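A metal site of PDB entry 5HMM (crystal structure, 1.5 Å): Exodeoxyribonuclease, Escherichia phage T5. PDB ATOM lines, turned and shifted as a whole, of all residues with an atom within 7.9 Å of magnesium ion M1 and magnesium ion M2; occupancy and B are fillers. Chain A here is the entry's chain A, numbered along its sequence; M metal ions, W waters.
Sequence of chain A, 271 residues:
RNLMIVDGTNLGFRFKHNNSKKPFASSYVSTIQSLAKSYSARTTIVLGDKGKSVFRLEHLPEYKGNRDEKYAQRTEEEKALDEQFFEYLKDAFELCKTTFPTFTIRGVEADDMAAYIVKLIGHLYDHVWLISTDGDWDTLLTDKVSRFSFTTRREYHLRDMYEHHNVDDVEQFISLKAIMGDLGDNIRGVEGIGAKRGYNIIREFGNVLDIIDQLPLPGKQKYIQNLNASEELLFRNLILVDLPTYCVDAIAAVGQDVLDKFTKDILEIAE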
ATOM      1  N   ASP A   7      10.762  35.804   7.509  1.00  0.00           N
ATOM      2  CA  ASP A   7      10.887  34.342   7.662  1.00  0.00           C
ATOM      3  C   ASP A   7      11.151  34.123   9.149  1.00  0.00           C
ATOM      4  O   ASP A   7      12.290  34.108   9.610  1.00  0.00           O
ATOM      5  CB  ASP A   7      12.033  33.828   6.798  1.00  0.00           C
ATOM      6  CG  ASP A   7      12.015  32.326   6.578  1.00  0.00           C
ATOM      7  OD1 ASP A   7      11.166  31.612   7.145  1.00  0.00           O
ATOM      8  OD2 ASP A   7      12.917  31.848   5.832  1.00  0.00           O
ATOM      9  N   THR A   9      10.560  31.765  11.629  1.00  0.00           N
ATOM     10  CA  THR A   9      11.209  30.593  12.262  1.00  0.00           C
ATOM     11  C   THR A   9      12.730  30.676  11.984  1.00  0.00           C
ATOM     12  O   THR A   9      13.552  30.445  12.862  1.00  0.00           O
ATOM     13  CB  THR A   9      10.588  29.278  11.783  1.00  0.00           C
ATOM     14  OG1 THR A   9       9.174  29.340  12.031  1.00  0.00           O
ATOM     15  CG2 THR A   9      11.176  28.085  12.492  1.00  0.00           C
ATOM     16  N   ASN A  10      13.041  31.065  10.753  1.00  0.00           N
ATOM     17  CA  ASN A  10      14.415  31.353  10.268  1.00  0.00           C
ATOM     18  C   ASN A  10      15.123  32.421  11.124  1.00  0.00           C
ATOM     19  O   ASN A  10      16.280  32.254  11.534  1.00  0.00           O
ATOM     20  CB  ASN A  10      14.337  31.753   8.778  1.00  0.00           C
ATOM     21  CG  ASN A  10      15.685  32.030   8.157  1.00  0.00           C
ATOM     22  OD1 ASN A  10      16.164  33.158   8.186  1.00  0.00           O
ATOM     23  ND2 ASN A  10      16.307  31.015   7.542  1.00  0.00           N
ATOM     24  N   GLY A  48       5.703  32.060  10.110  1.00  0.00           N
ATOM     25  CA  GLY A  48       6.376  30.965  10.788  1.00  0.00           C
ATOM     26  C   GLY A  48       6.036  29.630  10.166  1.00  0.00           C
ATOM     27  O   GLY A  48       5.038  29.505   9.455  1.00  0.00           O
ATOM     28  N   ASP A  49       6.893  28.655  10.410  1.00  0.00           N
ATOM     29  CA  ASP A  49       6.663  27.253  10.009  1.00  0.00           C
ATOM     30  C   ASP A  49       5.947  26.474  11.102  1.00  0.00           C
ATOM     31  O   ASP A  49       6.342  26.518  12.248  1.00  0.00           O
ATOM     32  CB  ASP A  49       7.963  26.584   9.604  1.00  0.00           C
ATOM     33  CG  ASP A  49       8.588  27.240   8.386  1.00  0.00           C
ATOM     34  OD1 ASP A  49       8.137  26.929   7.256  1.00  0.00           O
ATOM     35  OD2 ASP A  49       9.494  28.073   8.583  1.00  0.00           O
ATOM     36  N   ARG A  56       4.742  19.288  -0.405  1.00  0.00           N
ATOM     37  CA  ARG A  56       6.005  18.675  -0.859  1.00  0.00           C
ATOM     38  C   ARG A  56       6.130  17.187  -0.458  1.00  0.00           C
ATOM     39  O   ARG A  56       6.653  16.373  -1.232  1.00  0.00           O
ATOM     40  CB  ARG A  56       7.210  19.511  -0.459  1.00  0.00           C
ATOM     41  CG  ARG A  56       7.226  20.859  -1.176  1.00  0.00           C
ATOM     42  CD  ARG A  56       8.455  21.710  -0.886  1.00  0.00           C
ATOM     43  NE  ARG A  56       8.240  22.934  -1.644  1.00  0.00           N
ATOM     44  CZ  ARG A  56       7.447  23.938  -1.276  1.00  0.00           C
ATOM     45  NH1 ARG A  56       6.856  23.957  -0.062  1.00  0.00           N
ATOM     46  NH2 ARG A  56       7.252  24.959  -2.104  1.00  0.00           N
ATOM     47  N   TYR A  63      11.085  13.986   1.444  1.00  0.00           N
ATOM     48  CA  TYR A  63      11.419  15.430   1.582  1.00  0.00           C
ATOM     49  C   TYR A  63      11.868  15.742   3.017  1.00  0.00           C
ATOM     50  O   TYR A  63      11.184  15.387   3.967  1.00  0.00           O
ATOM     51  CB  TYR A  63      10.240  16.297   1.203  1.00  0.00           C
ATOM     52  CG  TYR A  63      10.437  17.790   1.310  1.00  0.00           C
ATOM     53  CD1 TYR A  63      11.281  18.485   0.431  1.00  0.00           C
ATOM     54  CD2 TYR A  63       9.762  18.528   2.275  1.00  0.00           C
ATOM     55  CE1 TYR A  63      11.436  19.857   0.515  1.00  0.00           C
ATOM     56  CE2 TYR A  63       9.913  19.909   2.368  1.00  0.00           C
ATOM     57  CZ  TYR A  63      10.758  20.559   1.486  1.00  0.00           C
ATOM     58  OH  TYR A  63      10.912  21.924   1.554  1.00  0.00           O
ATOM     59  N   LYS A  64      13.034  16.371   3.130  1.00  0.00           N
ATOM     60  CA  LYS A  64      13.661  16.696   4.426  1.00  0.00           C
ATOM     61  C   LYS A  64      13.834  15.468   5.352  1.00  0.00           C
ATOM     62  O   LYS A  64      13.891  15.591   6.580  1.00  0.00           O
ATOM     63  CB  LYS A  64      12.863  17.798   5.121  1.00  0.00           C
ATOM     64  CG  LYS A  64      12.986  19.140   4.415  1.00  0.00           C
ATOM     65  CD  LYS A  64      12.335  20.222   5.246  1.00  0.00           C
ATOM     66  CE  LYS A  64      12.484  21.587   4.604  1.00  0.00           C
ATOM     67  NZ  LYS A  64      11.946  22.606   5.539  1.00  0.00           N
ATOM     68  N   GLU A 109       4.606  25.575   4.493  1.00  0.00           N
ATOM     69  CA  GLU A 109       5.895  26.245   4.727  1.00  0.00           C
ATOM     70  C   GLU A 109       5.731  27.740   4.632  1.00  0.00           C
ATOM     71  O   GLU A 109       4.983  28.276   3.803  1.00  0.00           O
ATOM     72  CB  GLU A 109       6.967  25.812   3.721  1.00  0.00           C
ATOM     73  CG  GLU A 109       7.373  24.366   3.858  1.00  0.00           C
ATOM     74  CD  GLU A 109       8.676  24.017   3.146  1.00  0.00           C
ATOM     75  OE1 GLU A 109       8.651  23.107   2.302  1.00  0.00           O
ATOM     76  OE2 GLU A 109       9.734  24.640   3.386  1.00  0.00           O
ATOM     77  N   ALA A 110       6.490  28.439   5.456  1.00  0.00           N
ATOM     78  CA  ALA A 110       6.517  29.895   5.393  1.00  0.00           C
ATOM     79  C   ALA A 110       6.913  30.394   3.992  1.00  0.00           C
ATOM     80  O   ALA A 110       6.407  31.416   3.512  1.00  0.00           O
ATOM     81  CB  ALA A 110       7.422  30.492   6.462  1.00  0.00           C
ATOM     82  N   ASP A 111       7.799  29.640   3.338  1.00  0.00           N
ATOM     83  CA  ASP A 111       8.244  29.976   1.981  1.00  0.00           C
ATOM     84  C   ASP A 111       7.048  30.222   1.049  1.00  0.00           C
ATOM     85  O   ASP A 111       7.000  31.185   0.267  1.00  0.00           O
ATOM     86  CB  ASP A 111       9.039  28.826   1.364  1.00  0.00           C
ATOM     87  CG  ASP A 111      10.281  28.466   2.132  1.00  0.00           C
ATOM     88  OD1 ASP A 111      10.314  28.594   3.378  1.00  0.00           O
ATOM     89  OD2 ASP A 111      11.226  28.007   1.477  1.00  0.00           O
ATOM     90  N   ASP A 112       6.097  29.314   1.137  1.00  0.00           N
ATOM     91  CA  ASP A 112       4.897  29.366   0.273  1.00  0.00           C
ATOM     92  C   ASP A 112       3.983  30.549   0.613  1.00  0.00           C
ATOM     93  O   ASP A 112       3.445  31.217  -0.275  1.00  0.00           O
ATOM     94  CB  ASP A 112       4.107  28.082   0.377  1.00  0.00           C
ATOM     95  CG  ASP A 112       4.872  26.872  -0.126  1.00  0.00           C
ATOM     96  OD1 ASP A 112       5.291  26.873  -1.304  1.00  0.00           O
ATOM     97  OD2 ASP A 112       5.067  25.921   0.665  1.00  0.00           O
ATOM     98  N   SER A 132      15.226  36.894   5.442  1.00  0.00           N
ATOM     99  CA  SER A 132      15.523  35.468   5.460  1.00  0.00           C
ATOM    100  C   SER A 132      16.960  35.187   5.116  1.00  0.00           C
ATOM    101  O   SER A 132      17.528  35.785   4.214  1.00  0.00           O
ATOM    102  CB  SER A 132      14.615  34.696   4.470  1.00  0.00           C
ATOM    103  OG  SER A 132      14.866  33.291   4.555  1.00  0.00           O
ATOM    104  N   ASP A 134      17.581  32.179   4.011  1.00  0.00           N
ATOM    105  CA  ASP A 134      17.335  31.098   3.052  1.00  0.00           C
ATOM    106  C   ASP A 134      17.516  31.598   1.598  1.00  0.00           C
ATOM    107  O   ASP A 134      16.687  32.348   1.094  1.00  0.00           O
ATOM    108  CB  ASP A 134      15.925  30.504   3.266  1.00  0.00           C
ATOM    109  CG  ASP A 134      15.683  29.210   2.491  1.00  0.00           C
ATOM    110  OD1 ASP A 134      16.533  28.802   1.674  1.00  0.00           O
ATOM    111  OD2 ASP A 134      14.603  28.600   2.681  1.00  0.00           O
ATOM    112  N   GLY A 135      18.580  31.153   0.945  1.00  0.00           N
ATOM    113  CA  GLY A 135      18.795  31.403  -0.497  1.00  0.00           C
ATOM    114  C   GLY A 135      17.622  31.000  -1.404  1.00  0.00           C
ATOM    115  O   GLY A 135      17.417  31.619  -2.458  1.00  0.00           O
ATOM    116  N   ASP A 136      16.865  29.978  -1.001  1.00  0.00           N
ATOM    117  CA  ASP A 136      15.592  29.533  -1.689  1.00  0.00           C
ATOM    118  C   ASP A 136      14.664  30.705  -1.981  1.00  0.00           C
ATOM    119  O   ASP A 136      13.951  30.720  -2.977  1.00  0.00           O
ATOM    120  CB  ASP A 136      14.692  28.603  -0.854  1.00  0.00           C
ATOM    121  CG  ASP A 136      15.131  27.143  -0.824  1.00  0.00           C
ATOM    122  OD1 ASP A 136      16.168  26.763  -1.394  1.00  0.00           O
ATOM    123  OD2 ASP A 136      14.373  26.363  -0.182  1.00  0.00           O
ATOM    124  N   TRP A 137      14.604  31.631  -1.036  1.00  0.00           N
ATOM    125  CA  TRP A 137      13.717  32.819  -1.158  1.00  0.00           C
ATOM    126  C   TRP A 137      14.106  33.755  -2.313  1.00  0.00           C
ATOM    127  O   TRP A 137      13.319  34.622  -2.705  1.00  0.00           O
ATOM    128  CB  TRP A 137      13.622  33.575   0.166  1.00  0.00           C
ATOM    129  CG  TRP A 137      12.732  32.895   1.200  1.00  0.00           C
ATOM    130  CD1 TRP A 137      12.658  31.562   1.474  1.00  0.00           C
ATOM    131  CD2 TRP A 137      11.824  33.543   2.094  1.00  0.00           C
ATOM    132  NE1 TRP A 137      11.739  31.341   2.476  1.00  0.00           N
ATOM    133  CE2 TRP A 137      11.219  32.533   2.873  1.00  0.00           C
ATOM    134  CE3 TRP A 137      11.445  34.866   2.287  1.00  0.00           C
ATOM    135  CZ2 TRP A 137      10.253  32.834   3.854  1.00  0.00           C
ATOM    136  CZ3 TRP A 137      10.504  35.168   3.267  1.00  0.00           C
ATOM    137  CH2 TRP A 137       9.906  34.151   4.024  1.00  0.00           C
ATOM    138  N   LYS A 177      18.075  24.758  -9.725  1.00  0.00           N
ATOM    139  CA  LYS A 177      17.683  24.028  -8.495  1.00  0.00           C
ATOM    140  C   LYS A 177      17.008  22.710  -8.824  1.00  0.00           C
ATOM    141  O   LYS A 177      17.215  21.702  -8.154  1.00  0.00           O
ATOM    142  CB  LYS A 177      16.785  24.862  -7.587  1.00  0.00           C
ATOM    143  CG  LYS A 177      17.488  26.094  -7.075  1.00  0.00           C
ATOM    144  CD  LYS A 177      16.514  27.120  -6.532  1.00  0.00           C
ATOM    145  CE  LYS A 177      16.019  26.701  -5.168  1.00  0.00           C
ATOM    146  NZ  LYS A 177      15.081  27.710  -4.656  1.00  0.00           N
ATOM    147  N   ASP A 182      18.711  19.469  -3.973  1.00  0.00           N
ATOM    148  CA  ASP A 182      19.003  20.180  -2.727  1.00  0.00           C
ATOM    149  C   ASP A 182      19.363  19.151  -1.687  1.00  0.00           C
ATOM    150  O   ASP A 182      18.503  18.429  -1.184  1.00  0.00           O
ATOM    151  CB  ASP A 182      17.792  21.019  -2.299  1.00  0.00           C
ATOM    152  CG  ASP A 182      18.100  21.974  -1.150  1.00  0.00           C
ATOM    153  OD1 ASP A 182      18.553  21.517  -0.094  1.00  0.00           O
ATOM    154  OD2 ASP A 182      17.852  23.205  -1.303  1.00  0.00           O
ATOM    155  N   ASP A 185      17.682  19.415   1.829  1.00  0.00           N
ATOM    156  CA  ASP A 185      16.262  19.028   1.885  1.00  0.00           C
ATOM    157  C   ASP A 185      15.953  17.649   1.283  1.00  0.00           C
ATOM    158  O   ASP A 185      14.807  17.278   1.092  1.00  0.00           O
ATOM    159  CB  ASP A 185      15.404  20.124   1.281  1.00  0.00           C
ATOM    160  CG  ASP A 185      15.362  21.386   2.156  1.00  0.00           C
ATOM    161  OD1 ASP A 185      15.662  21.323   3.373  1.00  0.00           O
ATOM    162  OD2 ASP A 185      15.024  22.443   1.621  1.00  0.00           O
ATOM    163  N   LEU A 240       8.747  20.912  -6.683  1.00  0.00           N
ATOM    164  CA  LEU A 240       9.293  21.065  -5.311  1.00  0.00           C
ATOM    165  C   LEU A 240      10.004  22.397  -5.073  1.00  0.00           C
ATOM    166  O   LEU A 240       9.990  22.908  -3.948  1.00  0.00           O
ATOM    167  CB  LEU A 240      10.238  19.932  -4.953  1.00  0.00           C
ATOM    168  CG  LEU A 240       9.647  18.530  -4.870  1.00  0.00           C
ATOM    169  CD1 LEU A 240      10.794  17.556  -4.643  1.00  0.00           C
ATOM    170  CD2 LEU A 240       8.580  18.399  -3.802  1.00  0.00           C
ATOM    171  N   LEU A 243       8.918  27.904  -6.369  1.00  0.00           N
ATOM    172  CA  LEU A 243       8.150  28.513  -5.307  1.00  0.00           C
ATOM    173  C   LEU A 243       7.032  29.465  -5.816  1.00  0.00           C
ATOM    174  O   LEU A 243       5.896  29.343  -5.360  1.00  0.00           O
ATOM    175  CB  LEU A 243       9.101  29.191  -4.335  1.00  0.00           C
ATOM    176  CG  LEU A 243       8.459  29.793  -3.116  1.00  0.00           C
ATOM    177  CD1 LEU A 243       7.790  28.707  -2.266  1.00  0.00           C
ATOM    178  CD2 LEU A 243       9.527  30.526  -2.327  1.00  0.00           C
HETATM  179 MG    MG M   1      13.112  26.881   1.915  1.00  0.00          MG
HETATM  180 MG    MG M   2      11.553  27.853   4.971  1.00  0.00          MG
HETATM  181 MG    MG M   3      17.623  25.015   0.073  1.00  0.00          MG
HETATM  182  O   HOH W   1      10.147  26.406   5.361  1.00  0.00           O
HETATM  183  O   HOH W   2      12.708  26.995   6.412  1.00  0.00           O
HETATM  184  O   HOH W   3      12.485  26.694   3.685  1.00  0.00           O
HETATM  185  O   HOH W   4      12.919  29.379   4.640  1.00  0.00           O
HETATM  186  O   HOH W   5      10.635  29.088   6.321  1.00  0.00           O
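Within 4 Å of magnesium ion M2: Asp 111 and Asp 134.
Along chain A the residues within 4 Å of magnesium ion M2 span positions 111 to 134.
The nearest printed residue that does not touch magnesium ion M2 is Glu 109 (4.02 Å).
Magnesium ion M2 is bound by water W3 (2.0 Å), water W2 (2.0 Å), water W5 (2.0 Å), water W1 (2.1 Å), water W4 (2.1 Å) and the side-chain carboxylate (OD1) of Asp 111 (2.1 Å).
Of the 22 residues printed, 3 come within 4 Å of magnesium ion M1.
The nearest printed residue that does not touch magnesium ion M1 is Glu 109 (4.3 Å).
Water W5 bridges the side-chain carboxylate (OD1) of Asp 7 (2.7 Å) and the side-chain carboxylate (OD2) of Asp 49 (2.7 Å).
Water W1 lies within hydrogen-bond range of the side-chain carboxylate of Glu 109 (2.7 Å) and the side-chain carboxylate of Asp 49 (2.8 Å).
Water W4 bridges OD2 of Asp 7 (2.7 Å) and NE1 of Trp 137 (3.2 Å).
Magnesium ion M1 is bound by water W3 (1.9 Å), OD2 of Asp 111 (2.2 Å), OD2 of Asp 134 (2.4 Å) and OD2 of Asp 136 (2.5 Å).
Magnesium ion M1 has four donor atoms within binding distance.
The side-chain carboxylate (OD1) of Asp 136 lies within salt-bridge range of the side-chain amino group (NZ) of Lys 177, at 3.6 Å.
The indole nitrogen of Trp 137 sits close to the side-chain carboxylate of Asp 111, at 3.2 Å.
The backbone NH (N) of Asp 134 is in hydrogen-bond range of the side-chain hydroxyl (OG) of Ser 132, at 3.0 Å.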
